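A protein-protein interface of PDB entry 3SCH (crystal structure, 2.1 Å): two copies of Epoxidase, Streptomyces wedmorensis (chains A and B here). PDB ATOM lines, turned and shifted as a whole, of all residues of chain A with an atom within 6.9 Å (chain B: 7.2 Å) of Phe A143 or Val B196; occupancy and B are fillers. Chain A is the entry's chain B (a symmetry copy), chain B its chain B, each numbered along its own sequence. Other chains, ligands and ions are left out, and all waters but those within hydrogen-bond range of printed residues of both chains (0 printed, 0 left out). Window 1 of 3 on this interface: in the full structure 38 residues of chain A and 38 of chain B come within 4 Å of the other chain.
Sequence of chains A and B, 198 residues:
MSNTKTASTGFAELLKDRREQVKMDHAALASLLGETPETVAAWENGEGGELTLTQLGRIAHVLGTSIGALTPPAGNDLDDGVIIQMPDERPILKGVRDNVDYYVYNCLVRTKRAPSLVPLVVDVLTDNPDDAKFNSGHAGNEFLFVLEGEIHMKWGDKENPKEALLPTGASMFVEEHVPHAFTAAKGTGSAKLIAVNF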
ATOM      1  N   LEU A 117      -7.236  29.156 -11.604  1.00  0.00           N
ATOM      2  CA  LEU A 117      -6.548  29.502 -10.373  1.00  0.00           C
ATOM      3  C   LEU A 117      -7.091  30.798  -9.789  1.00  0.00           C
ATOM      4  O   LEU A 117      -6.949  31.871 -10.394  1.00  0.00           O
ATOM      5  CB  LEU A 117      -5.048  29.654 -10.612  1.00  0.00           C
ATOM      6  CG  LEU A 117      -4.252  30.281  -9.461  1.00  0.00           C
ATOM      7  CD1 LEU A 117      -4.246  29.325  -8.258  1.00  0.00           C
ATOM      8  CD2 LEU A 117      -2.813  30.558  -9.926  1.00  0.00           C
ATOM      9  N   ASN A 141     -11.578  22.233  -7.559  1.00  0.00           N
ATOM     10  CA  ASN A 141     -11.068  21.875  -6.252  1.00  0.00           C
ATOM     11  C   ASN A 141     -10.558  23.085  -5.502  1.00  0.00           C
ATOM     12  O   ASN A 141     -10.216  24.102  -6.094  1.00  0.00           O
ATOM     13  CB  ASN A 141      -9.936  20.878  -6.392  1.00  0.00           C
ATOM     14  CG  ASN A 141     -10.383  19.592  -7.026  1.00  0.00           C
ATOM     15  OD1 ASN A 141     -11.499  19.127  -6.788  1.00  0.00           O
ATOM     16  ND2 ASN A 141      -9.507  18.995  -7.828  1.00  0.00           N
ATOM     17  N   GLU A 142     -10.476  22.962  -4.188  1.00  0.00           N
ATOM     18  CA  GLU A 142     -10.010  24.071  -3.383  1.00  0.00           C
ATOM     19  C   GLU A 142      -9.102  23.587  -2.274  1.00  0.00           C
ATOM     20  O   GLU A 142      -9.435  22.629  -1.554  1.00  0.00           O
ATOM     21  CB  GLU A 142     -11.210  24.817  -2.798  1.00  0.00           C
ATOM     22  CG  GLU A 142     -10.845  26.061  -1.973  1.00  0.00           C
ATOM     23  CD  GLU A 142     -12.069  26.849  -1.523  1.00  0.00           C
ATOM     24  OE1 GLU A 142     -13.153  26.257  -1.331  1.00  0.00           O
ATOM     25  OE2 GLU A 142     -11.945  28.074  -1.338  1.00  0.00           O
ATOM     26  N   PHE A 143      -7.940  24.227  -2.172  1.00  0.00           N
ATOM     27  CA  PHE A 143      -6.963  23.939  -1.133  1.00  0.00           C
ATOM     28  C   PHE A 143      -7.034  25.111  -0.162  1.00  0.00           C
ATOM     29  O   PHE A 143      -7.124  26.266  -0.591  1.00  0.00           O
ATOM     30  CB  PHE A 143      -5.540  23.857  -1.698  1.00  0.00           C
ATOM     31  CG  PHE A 143      -4.451  24.030  -0.650  1.00  0.00           C
ATOM     32  CD1 PHE A 143      -4.093  22.979   0.199  1.00  0.00           C
ATOM     33  CD2 PHE A 143      -3.795  25.257  -0.501  1.00  0.00           C
ATOM     34  CE1 PHE A 143      -3.104  23.146   1.178  1.00  0.00           C
ATOM     35  CE2 PHE A 143      -2.806  25.429   0.478  1.00  0.00           C
ATOM     36  CZ  PHE A 143      -2.460  24.373   1.319  1.00  0.00           C
ATOM     37  N   LEU A 144      -7.016  24.817   1.138  1.00  0.00           N
ATOM     38  CA  LEU A 144      -7.073  25.876   2.139  1.00  0.00           C
ATOM     39  C   LEU A 144      -6.017  25.683   3.194  1.00  0.00           C
ATOM     40  O   LEU A 144      -5.601  24.560   3.465  1.00  0.00           O
ATOM     41  CB  LEU A 144      -8.446  25.944   2.812  1.00  0.00           C
ATOM     42  CG  LEU A 144      -9.588  26.218   1.835  1.00  0.00           C
ATOM     43  CD1 LEU A 144     -10.280  24.903   1.521  1.00  0.00           C
ATOM     44  CD2 LEU A 144     -10.573  27.226   2.430  1.00  0.00           C
ATOM     45  N   PHE A 145      -5.610  26.801   3.793  1.00  0.00           N
ATOM     46  CA  PHE A 145      -4.589  26.843   4.836  1.00  0.00           C
ATOM     47  C   PHE A 145      -5.054  27.898   5.860  1.00  0.00           C
ATOM     48  O   PHE A 145      -5.434  29.002   5.469  1.00  0.00           O
ATOM     49  CB  PHE A 145      -3.256  27.279   4.223  1.00  0.00           C
ATOM     50  CG  PHE A 145      -2.116  27.363   5.213  1.00  0.00           C
ATOM     51  CD1 PHE A 145      -1.386  26.230   5.553  1.00  0.00           C
ATOM     52  CD2 PHE A 145      -1.753  28.584   5.772  1.00  0.00           C
ATOM     53  CE1 PHE A 145      -0.296  26.308   6.436  1.00  0.00           C
ATOM     54  CE2 PHE A 145      -0.659  28.680   6.662  1.00  0.00           C
ATOM     55  CZ  PHE A 145       0.070  27.539   6.990  1.00  0.00           C
ATOM     56  N   ALA A 170      -3.194  24.525   9.960  1.00  0.00           N
ATOM     57  CA  ALA A 170      -3.925  23.367   9.428  1.00  0.00           C
ATOM     58  C   ALA A 170      -4.178  23.566   7.933  1.00  0.00           C
ATOM     59  O   ALA A 170      -4.313  24.697   7.468  1.00  0.00           O
ATOM     60  CB  ALA A 170      -5.256  23.209  10.140  1.00  0.00           C
ATOM     61  N   SER A 171      -4.257  22.472   7.184  1.00  0.00           N
ATOM     62  CA  SER A 171      -4.537  22.582   5.753  1.00  0.00           C
ATOM     63  C   SER A 171      -5.691  21.658   5.375  1.00  0.00           C
ATOM     64  O   SER A 171      -5.941  20.642   6.029  1.00  0.00           O
ATOM     65  CB  SER A 171      -3.275  22.295   4.910  1.00  0.00           C
ATOM     66  OG  SER A 171      -2.766  20.985   5.074  1.00  0.00           O
ATOM     67  N   MET A 172      -6.408  22.018   4.326  1.00  0.00           N
ATOM     68  CA  MET A 172      -7.541  21.219   3.907  1.00  0.00           C
ATOM     69  C   MET A 172      -7.725  21.190   2.387  1.00  0.00           C
ATOM     70  O   MET A 172      -7.276  22.082   1.666  1.00  0.00           O
ATOM     71  CB  MET A 172      -8.822  21.767   4.541  1.00  0.00           C
ATOM     72  CG  MET A 172      -8.712  22.134   6.021  1.00  0.00           C
ATOM     73  SD  MET A 172      -7.982  23.924   6.357  1.00  0.00           S
ATOM     74  CE  MET A 172      -9.664  24.887   6.276  1.00  0.00           C
ATOM     75  N   PHE A 173      -8.378  20.144   1.912  1.00  0.00           N
ATOM     76  CA  PHE A 173      -8.687  20.031   0.501  1.00  0.00           C
ATOM     77  C   PHE A 173     -10.183  19.783   0.419  1.00  0.00           C
ATOM     78  O   PHE A 173     -10.714  18.922   1.130  1.00  0.00           O
ATOM     79  CB  PHE A 173      -7.932  18.862  -0.139  1.00  0.00           C
ATOM     80  CG  PHE A 173      -8.425  18.516  -1.521  1.00  0.00           C
ATOM     81  CD1 PHE A 173      -7.896  19.143  -2.643  1.00  0.00           C
ATOM     82  CD2 PHE A 173      -9.448  17.584  -1.695  1.00  0.00           C
ATOM     83  CE1 PHE A 173      -8.382  18.851  -3.920  1.00  0.00           C
ATOM     84  CE2 PHE A 173      -9.935  17.287  -2.965  1.00  0.00           C
ATOM     85  CZ  PHE A 173      -9.401  17.923  -4.080  1.00  0.00           C
ATOM     86  N   VAL A 174     -10.866  20.546  -0.424  1.00  0.00           N
ATOM     87  CA  VAL A 174     -12.304  20.390  -0.607  1.00  0.00           C
ATOM     88  C   VAL A 174     -12.555  20.114  -2.088  1.00  0.00           C
ATOM     89  O   VAL A 174     -12.244  20.945  -2.941  1.00  0.00           O
ATOM     90  CB  VAL A 174     -13.092  21.674  -0.198  1.00  0.00           C
ATOM     91  CG1 VAL A 174     -14.590  21.418  -0.321  1.00  0.00           C
ATOM     92  CG2 VAL A 174     -12.733  22.089   1.224  1.00  0.00           C
ATOM     93  N   ILE A 194      -6.141  31.061   3.711  1.00  0.00           N
ATOM     94  CA  ILE A 194      -5.605  31.288   2.377  1.00  0.00           C
ATOM     95  C   ILE A 194      -6.424  30.209   1.664  1.00  0.00           C
ATOM     96  O   ILE A 194      -6.373  29.037   2.065  1.00  0.00           O
ATOM     97  CB  ILE A 194      -4.189  30.828   2.156  1.00  0.00           C
ATOM     98  CG1 ILE A 194      -3.193  31.755   2.822  1.00  0.00           C
ATOM     99  CG2 ILE A 194      -3.935  30.829   0.626  1.00  0.00           C
ATOM    100  CD1 ILE A 194      -2.918  33.007   2.011  1.00  0.00           C
ATOM    101  N   ALA A 195      -7.181  30.589   0.643  1.00  0.00           N
ATOM    102  CA  ALA A 195      -7.999  29.635  -0.092  1.00  0.00           C
ATOM    103  C   ALA A 195      -7.517  29.674  -1.532  1.00  0.00           C
ATOM    104  O   ALA A 195      -7.457  30.749  -2.143  1.00  0.00           O
ATOM    105  CB  ALA A 195      -9.474  30.040  -0.028  1.00  0.00           C
ATOM    106  N   VAL A 196      -7.165  28.509  -2.063  1.00  0.00           N
ATOM    107  CA  VAL A 196      -6.681  28.432  -3.433  1.00  0.00           C
ATOM    108  C   VAL A 196      -7.590  27.549  -4.285  1.00  0.00           C
ATOM    109  O   VAL A 196      -7.575  26.329  -4.179  1.00  0.00           O
ATOM    110  CB  VAL A 196      -5.251  27.875  -3.485  1.00  0.00           C
ATOM    111  CG1 VAL A 196      -4.768  27.811  -4.926  1.00  0.00           C
ATOM    112  CG2 VAL A 196      -4.324  28.751  -2.668  1.00  0.00           C
ATOM    113  N   ASN A 197      -8.409  28.190  -5.103  1.00  0.00           N
ATOM    114  CA  ASN A 197      -9.289  27.476  -6.000  1.00  0.00           C
ATOM    115  C   ASN A 197      -8.419  27.097  -7.183  1.00  0.00           C
ATOM    116  O   ASN A 197      -7.601  27.898  -7.621  1.00  0.00           O
ATOM    117  CB  ASN A 197     -10.422  28.389  -6.475  1.00  0.00           C
ATOM    118  CG  ASN A 197     -11.404  28.714  -5.363  1.00  0.00           C
ATOM    119  OD1 ASN A 197     -12.148  27.841  -4.913  1.00  0.00           O
ATOM    120  ND2 ASN A 197     -11.404  29.977  -4.903  1.00  0.00           N
ATOM    121  N   PHE A 198      -8.561  25.876  -7.682  1.00  0.00           N
ATOM    122  CA  PHE A 198      -7.775  25.475  -8.836  1.00  0.00           C
ATOM    123  C   PHE A 198      -8.508  24.407  -9.633  1.00  0.00           C
ATOM    124  O   PHE A 198      -9.589  23.965  -9.180  1.00  0.00           O
ATOM    125  CB  PHE A 198      -6.360  24.999  -8.426  1.00  0.00           C
ATOM    126  CG  PHE A 198      -6.331  23.723  -7.621  1.00  0.00           C
ATOM    127  CD1 PHE A 198      -6.549  23.739  -6.249  1.00  0.00           C
ATOM    128  CD2 PHE A 198      -6.073  22.498  -8.239  1.00  0.00           C
ATOM    129  CE1 PHE A 198      -6.509  22.563  -5.504  1.00  0.00           C
ATOM    130  CE2 PHE A 198      -6.030  21.310  -7.504  1.00  0.00           C
ATOM    131  CZ  PHE A 198      -6.249  21.342  -6.133  1.00  0.00           C
ATOM    132  OXT PHE A 198      -8.007  24.045 -10.714  1.00  0.00           O
ATOM    133  N   LEU B 108       2.104  19.908   3.354  1.00  0.00           N
ATOM    134  CA  LEU B 108       0.740  20.116   3.797  1.00  0.00           C
ATOM    135  C   LEU B 108      -0.116  19.001   3.190  1.00  0.00           C
ATOM    136  O   LEU B 108       0.404  18.096   2.549  1.00  0.00           O
ATOM    137  CB  LEU B 108       0.245  21.506   3.364  1.00  0.00           C
ATOM    138  CG  LEU B 108       1.145  22.630   3.876  1.00  0.00           C
ATOM    139  CD1 LEU B 108       0.717  23.967   3.278  1.00  0.00           C
ATOM    140  CD2 LEU B 108       1.080  22.650   5.398  1.00  0.00           C
ATOM    141  N   VAL B 109      -1.425  19.086   3.381  1.00  0.00           N
ATOM    142  CA  VAL B 109      -2.349  18.067   2.910  1.00  0.00           C
ATOM    143  C   VAL B 109      -2.285  17.719   1.422  1.00  0.00           C
ATOM    144  O   VAL B 109      -2.133  18.594   0.571  1.00  0.00           O
ATOM    145  CB  VAL B 109      -3.808  18.471   3.254  1.00  0.00           C
ATOM    146  CG1 VAL B 109      -4.310  19.538   2.278  1.00  0.00           C
ATOM    147  CG2 VAL B 109      -4.717  17.241   3.221  1.00  0.00           C
ATOM    148  N   ARG B 110      -2.432  16.426   1.130  1.00  0.00           N
ATOM    149  CA  ARG B 110      -2.446  15.908  -0.243  1.00  0.00           C
ATOM    150  C   ARG B 110      -3.616  14.922  -0.385  1.00  0.00           C
ATOM    151  O   ARG B 110      -4.164  14.448   0.605  1.00  0.00           O
ATOM    152  CB  ARG B 110      -1.126  15.188  -0.586  1.00  0.00           C
ATOM    153  CG  ARG B 110       0.092  16.094  -0.723  1.00  0.00           C
ATOM    154  CD  ARG B 110       1.192  15.443  -1.563  1.00  0.00           C
ATOM    155  NE  ARG B 110       1.869  14.291  -0.949  1.00  0.00           N
ATOM    156  CZ  ARG B 110       2.961  14.362  -0.191  1.00  0.00           C
ATOM    157  NH1 ARG B 110       3.503  13.263   0.296  1.00  0.00           N
ATOM    158  NH2 ARG B 110       3.514  15.531   0.092  1.00  0.00           N
ATOM    159  N   SER B 116      -1.749  15.857  -8.527  1.00  0.00           N
ATOM    160  CA  SER B 116      -0.776  16.920  -8.803  1.00  0.00           C
ATOM    161  C   SER B 116      -0.713  18.008  -7.726  1.00  0.00           C
ATOM    162  O   SER B 116       0.183  18.860  -7.738  1.00  0.00           O
ATOM    163  CB  SER B 116      -1.031  17.557 -10.185  1.00  0.00           C
ATOM    164  OG  SER B 116      -2.267  18.257 -10.236  1.00  0.00           O
ATOM    165  N   LEU B 117      -1.644  17.977  -6.779  1.00  0.00           N
ATOM    166  CA  LEU B 117      -1.623  18.974  -5.723  1.00  0.00           C
ATOM    167  C   LEU B 117      -0.573  18.636  -4.674  1.00  0.00           C
ATOM    168  O   LEU B 117      -0.686  17.618  -3.974  1.00  0.00           O
ATOM    169  CB  LEU B 117      -2.986  19.079  -5.046  1.00  0.00           C
ATOM    170  CG  LEU B 117      -3.022  19.890  -3.745  1.00  0.00           C
ATOM    171  CD1 LEU B 117      -2.751  21.370  -4.054  1.00  0.00           C
ATOM    172  CD2 LEU B 117      -4.400  19.730  -3.080  1.00  0.00           C
ATOM    173  N   VAL B 118       0.451  19.481  -4.570  1.00  0.00           N
ATOM    174  CA  VAL B 118       1.499  19.295  -3.573  1.00  0.00           C
ATOM    175  C   VAL B 118       1.764  20.644  -2.893  1.00  0.00           C
ATOM    176  O   VAL B 118       2.598  21.426  -3.341  1.00  0.00           O
ATOM    177  CB  VAL B 118       2.813  18.787  -4.195  1.00  0.00           C
ATOM    178  CG1 VAL B 118       3.820  18.512  -3.072  1.00  0.00           C
ATOM    179  CG2 VAL B 118       2.564  17.500  -5.012  1.00  0.00           C
ATOM    180  N   PRO B 119       1.030  20.938  -1.810  1.00  0.00           N
ATOM    181  CA  PRO B 119       1.175  22.195  -1.063  1.00  0.00           C
ATOM    182  C   PRO B 119       2.228  22.025   0.022  1.00  0.00           C
ATOM    183  O   PRO B 119       2.334  20.959   0.631  1.00  0.00           O
ATOM    184  CB  PRO B 119      -0.225  22.423  -0.508  1.00  0.00           C
ATOM    185  CG  PRO B 119      -0.674  21.038  -0.179  1.00  0.00           C
ATOM    186  CD  PRO B 119      -0.082  20.135  -1.277  1.00  0.00           C
ATOM    187  N   LEU B 120       2.997  23.079   0.263  1.00  0.00           N
ATOM    188  CA  LEU B 120       4.079  23.022   1.225  1.00  0.00           C
ATOM    189  C   LEU B 120       4.319  24.391   1.842  1.00  0.00           C
ATOM    190  O   LEU B 120       3.975  25.429   1.249  1.00  0.00           O
ATOM    191  CB  LEU B 120       5.375  22.651   0.507  1.00  0.00           C
ATOM    192  CG  LEU B 120       5.447  21.577  -0.572  1.00  0.00           C
ATOM    193  CD1 LEU B 120       6.582  21.890  -1.558  1.00  0.00           C
ATOM    194  CD2 LEU B 120       5.682  20.244   0.086  1.00  0.00           C
ATOM    195  N   ASN B 141       2.111  23.790 -12.717  1.00  0.00           N
ATOM    196  CA  ASN B 141       2.142  25.171 -12.282  1.00  0.00           C
ATOM    197  C   ASN B 141       2.329  25.279 -10.785  1.00  0.00           C
ATOM    198  O   ASN B 141       2.034  24.352 -10.039  1.00  0.00           O
ATOM    199  CB  ASN B 141       0.849  25.863 -12.661  1.00  0.00           C
ATOM    200  CG  ASN B 141       0.638  25.905 -14.147  1.00  0.00           C
ATOM    201  OD1 ASN B 141       1.591  26.060 -14.914  1.00  0.00           O
ATOM    202  ND2 ASN B 141      -0.617  25.784 -14.568  1.00  0.00           N
ATOM    203  N   GLU B 142       2.792  26.434 -10.339  1.00  0.00           N
ATOM    204  CA  GLU B 142       3.015  26.628  -8.922  1.00  0.00           C
ATOM    205  C   GLU B 142       2.584  28.014  -8.495  1.00  0.00           C
ATOM    206  O   GLU B 142       2.940  29.017  -9.139  1.00  0.00           O
ATOM    207  CB  GLU B 142       4.495  26.412  -8.604  1.00  0.00           C
ATOM    208  CG  GLU B 142       4.849  26.528  -7.113  1.00  0.00           C
ATOM    209  CD  GLU B 142       6.302  26.174  -6.823  1.00  0.00           C
ATOM    210  OE1 GLU B 142       7.174  26.365  -7.698  1.00  0.00           O
ATOM    211  OE2 GLU B 142       6.584  25.716  -5.700  1.00  0.00           O
ATOM    212  N   PHE B 143       1.782  28.056  -7.434  1.00  0.00           N
ATOM    213  CA  PHE B 143       1.311  29.301  -6.844  1.00  0.00           C
ATOM    214  C   PHE B 143       2.086  29.461  -5.543  1.00  0.00           C
ATOM    215  O   PHE B 143       2.271  28.486  -4.806  1.00  0.00           O
ATOM    216  CB  PHE B 143      -0.187  29.242  -6.518  1.00  0.00           C
ATOM    217  CG  PHE B 143      -0.636  30.281  -5.501  1.00  0.00           C
ATOM    218  CD1 PHE B 143      -0.845  31.611  -5.873  1.00  0.00           C
ATOM    219  CD2 PHE B 143      -0.830  29.927  -4.160  1.00  0.00           C
ATOM    220  CE1 PHE B 143      -1.239  32.572  -4.931  1.00  0.00           C
ATOM    221  CE2 PHE B 143      -1.221  30.886  -3.215  1.00  0.00           C
ATOM    222  CZ  PHE B 143      -1.426  32.209  -3.599  1.00  0.00           C
ATOM    223  N   LEU B 144       2.556  30.679  -5.269  1.00  0.00           N
ATOM    224  CA  LEU B 144       3.304  30.926  -4.042  1.00  0.00           C
ATOM    225  C   LEU B 144       2.794  32.154  -3.335  1.00  0.00           C
ATOM    226  O   LEU B 144       2.267  33.065  -3.965  1.00  0.00           O
ATOM    227  CB  LEU B 144       4.801  31.093  -4.317  1.00  0.00           C
ATOM    228  CG  LEU B 144       5.439  29.866  -4.964  1.00  0.00           C
ATOM    229  CD1 LEU B 144       5.571  30.121  -6.456  1.00  0.00           C
ATOM    230  CD2 LEU B 144       6.803  29.575  -4.337  1.00  0.00           C
ATOM    231  N   PHE B 145       2.981  32.161  -2.015  1.00  0.00           N
ATOM    232  CA  PHE B 145       2.557  33.247  -1.137  1.00  0.00           C
ATOM    233  C   PHE B 145       3.667  33.413  -0.080  1.00  0.00           C
ATOM    234  O   PHE B 145       4.108  32.422   0.505  1.00  0.00           O
ATOM    235  CB  PHE B 145       1.248  32.857  -0.445  1.00  0.00           C
ATOM    236  CG  PHE B 145       0.708  33.907   0.498  1.00  0.00           C
ATOM    237  CD1 PHE B 145      -0.065  34.961   0.021  1.00  0.00           C
ATOM    238  CD2 PHE B 145       0.942  33.817   1.867  1.00  0.00           C
ATOM    239  CE1 PHE B 145      -0.610  35.913   0.897  1.00  0.00           C
ATOM    240  CE2 PHE B 145       0.402  34.767   2.761  1.00  0.00           C
ATOM    241  CZ  PHE B 145      -0.377  35.815   2.273  1.00  0.00           C
ATOM    242  N   ILE B 194       4.482  29.736   1.195  1.00  0.00           N
ATOM    243  CA  ILE B 194       3.501  28.666   1.092  1.00  0.00           C
ATOM    244  C   ILE B 194       3.632  28.442  -0.417  1.00  0.00           C
ATOM    245  O   ILE B 194       3.464  29.393  -1.195  1.00  0.00           O
ATOM    246  CB  ILE B 194       2.062  29.084   1.241  1.00  0.00           C
ATOM    247  CG1 ILE B 194       1.721  29.394   2.684  1.00  0.00           C
ATOM    248  CG2 ILE B 194       1.185  27.901   0.756  1.00  0.00           C
ATOM    249  CD1 ILE B 194       1.450  28.149   3.507  1.00  0.00           C
ATOM    250  N   ALA B 195       3.943  27.221  -0.830  1.00  0.00           N
ATOM    251  CA  ALA B 195       4.095  26.913  -2.245  1.00  0.00           C
ATOM    252  C   ALA B 195       3.067  25.842  -2.565  1.00  0.00           C
ATOM    253  O   ALA B 195       3.024  24.798  -1.901  1.00  0.00           O
ATOM    254  CB  ALA B 195       5.503  26.381  -2.526  1.00  0.00           C
ATOM    255  N   VAL B 196       2.239  26.106  -3.568  1.00  0.00           N
ATOM    256  CA  VAL B 196       1.210  25.152  -3.956  1.00  0.00           C
ATOM    257  C   VAL B 196       1.409  24.689  -5.398  1.00  0.00           C
ATOM    258  O   VAL B 196       1.132  25.417  -6.344  1.00  0.00           O
ATOM    259  CB  VAL B 196      -0.192  25.762  -3.814  1.00  0.00           C
ATOM    260  CG1 VAL B 196      -1.247  24.743  -4.218  1.00  0.00           C
ATOM    261  CG2 VAL B 196      -0.421  26.204  -2.383  1.00  0.00           C
ATOM    262  N   ASN B 197       1.928  23.481  -5.546  1.00  0.00           N
ATOM    263  CA  ASN B 197       2.124  22.901  -6.855  1.00  0.00           C
ATOM    264  C   ASN B 197       0.765  22.355  -7.248  1.00  0.00           C
ATOM    265  O   ASN B 197       0.069  21.787  -6.414  1.00  0.00           O
ATOM    266  CB  ASN B 197       3.132  21.752  -6.783  1.00  0.00           C
ATOM    267  CG  ASN B 197       4.544  22.239  -6.510  1.00  0.00           C
ATOM    268  OD1 ASN B 197       5.162  22.874  -7.366  1.00  0.00           O
ATOM    269  ND2 ASN B 197       5.060  21.955  -5.302  1.00  0.00           N
ATOM    270  N   PHE B 198       0.365  22.550  -8.498  1.00  0.00           N
ATOM    271  CA  PHE B 198      -0.915  22.018  -8.935  1.00  0.00           C
ATOM    272  C   PHE B 198      -0.893  21.741 -10.430  1.00  0.00           C
ATOM    273  O   PHE B 198       0.127  22.068 -11.080  1.00  0.00           O
ATOM    274  CB  PHE B 198      -2.085  22.957  -8.554  1.00  0.00           C
ATOM    275  CG  PHE B 198      -2.085  24.287  -9.268  1.00  0.00           C
ATOM    276  CD1 PHE B 198      -1.302  25.341  -8.816  1.00  0.00           C
ATOM    277  CD2 PHE B 198      -2.885  24.488 -10.396  1.00  0.00           C
ATOM    278  CE1 PHE B 198      -1.313  26.572  -9.468  1.00  0.00           C
ATOM    279  CE2 PHE B 198      -2.906  25.718 -11.059  1.00  0.00           C
ATOM    280  CZ  PHE B 198      -2.118  26.763 -10.595  1.00  0.00           C
ATOM    281  OXT PHE B 198      -1.883  21.176 -10.929  1.00  0.00           O
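Among the printed residues, pairs that only touch across the chains: Leu A117 with Phe B198 (3.9 Å), Phe A143 with Leu B108 (3.8 Å), Phe A143 with Val B109 (3.96 Å), Phe A143 with Pro B119 (3.4 Å), Phe A143 with Val B196 (3.8 Å), Phe A145 with Leu B108 (3.8 Å), Phe A145 with Ile B194 (3.8 Å), Ser A171 with Leu B108 (3.5 Å), Met A172 with Val B109 (3.8 Å), Phe A173 with Leu B117 (3.6 Å), Ile A194 with Phe B145 (3.8 Å), Val A196 with Phe B143 (3.8 Å) and Phe A198 with Leu B117 (3.9 Å).
Phe A143 touches just these residues of chain B: Leu B108, Val B109, Pro B119 and Val B196. Printed residues of chain B within 4 Å of Met A172: Val B109. Printed residues of chain A within 4 Å of Leu B108: Phe A143 (3.8 Å), Phe A145 (3.8 Å) and Ser A171 (3.5 Å). Of the printed residues of chain B, Phe A198 touches Leu B117. The nearest residue of chain B that does not touch Phe A143 is Leu B117 (4.4 Å). The nearest printed residue of chain A that does not touch Phe B143 is Leu A117 (4.4 Å).
The backbone NH (N) of Val B109 is in hydrogen-bond range of the side-chain hydroxyl (OG) of Ser A171.
Hydrophobic or aromatic side chains of chain A within 4 Å of the printed part of chain B: Leu A117, Phe A143, Phe A145, Phe A173, Ile A194, Val A196 and Phe A198. Along chain A the printed residues that touch a printed residue of chain B span positions 117 to 198. Among the printed residues, no Asp or Glu carboxylate lies within 4 Å of a Lys or Arg side-chain nitrogen of the other chain.
The backbone NH of Leu B108 is in hydrogen-bond range of the backbone carbonyl oxygen of Pro B119 (2.9 Å). The backbone carbonyl oxygen (O) of Asn B141 sits at hydrogen-bond distance from the backbone NH (N) of Phe B198, at 2.9 Å. O of Phe B143 is in hydrogen-bond range of N of Val B196, 2.7 Å away. The backbone NH (N) of Phe A198 sits at hydrogen-bond distance from the backbone carbonyl oxygen (O) of Asn A141. O of Phe A143 is in hydrogen-bond range of N of Val A196 (2.7 Å). The backbone NH (N) of Leu A144 is in hydrogen-bond range of the backbone carbonyl oxygen (O) of Met A172, at 2.8 Å.
Leu A117 touches Phe B198, and with the chains exchanged Phe A198 touches Leu B117. Phe A143 touches Val B196, and with the chains exchanged Val A196 touches Phe B143. Phe A145 touches Ile B194, and with the chains exchanged Ile A194 touches Phe B145. Positions printed for both chains: 117, 141, 142, 143, 144, 145, 194, 195, 196, 197 and 198.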
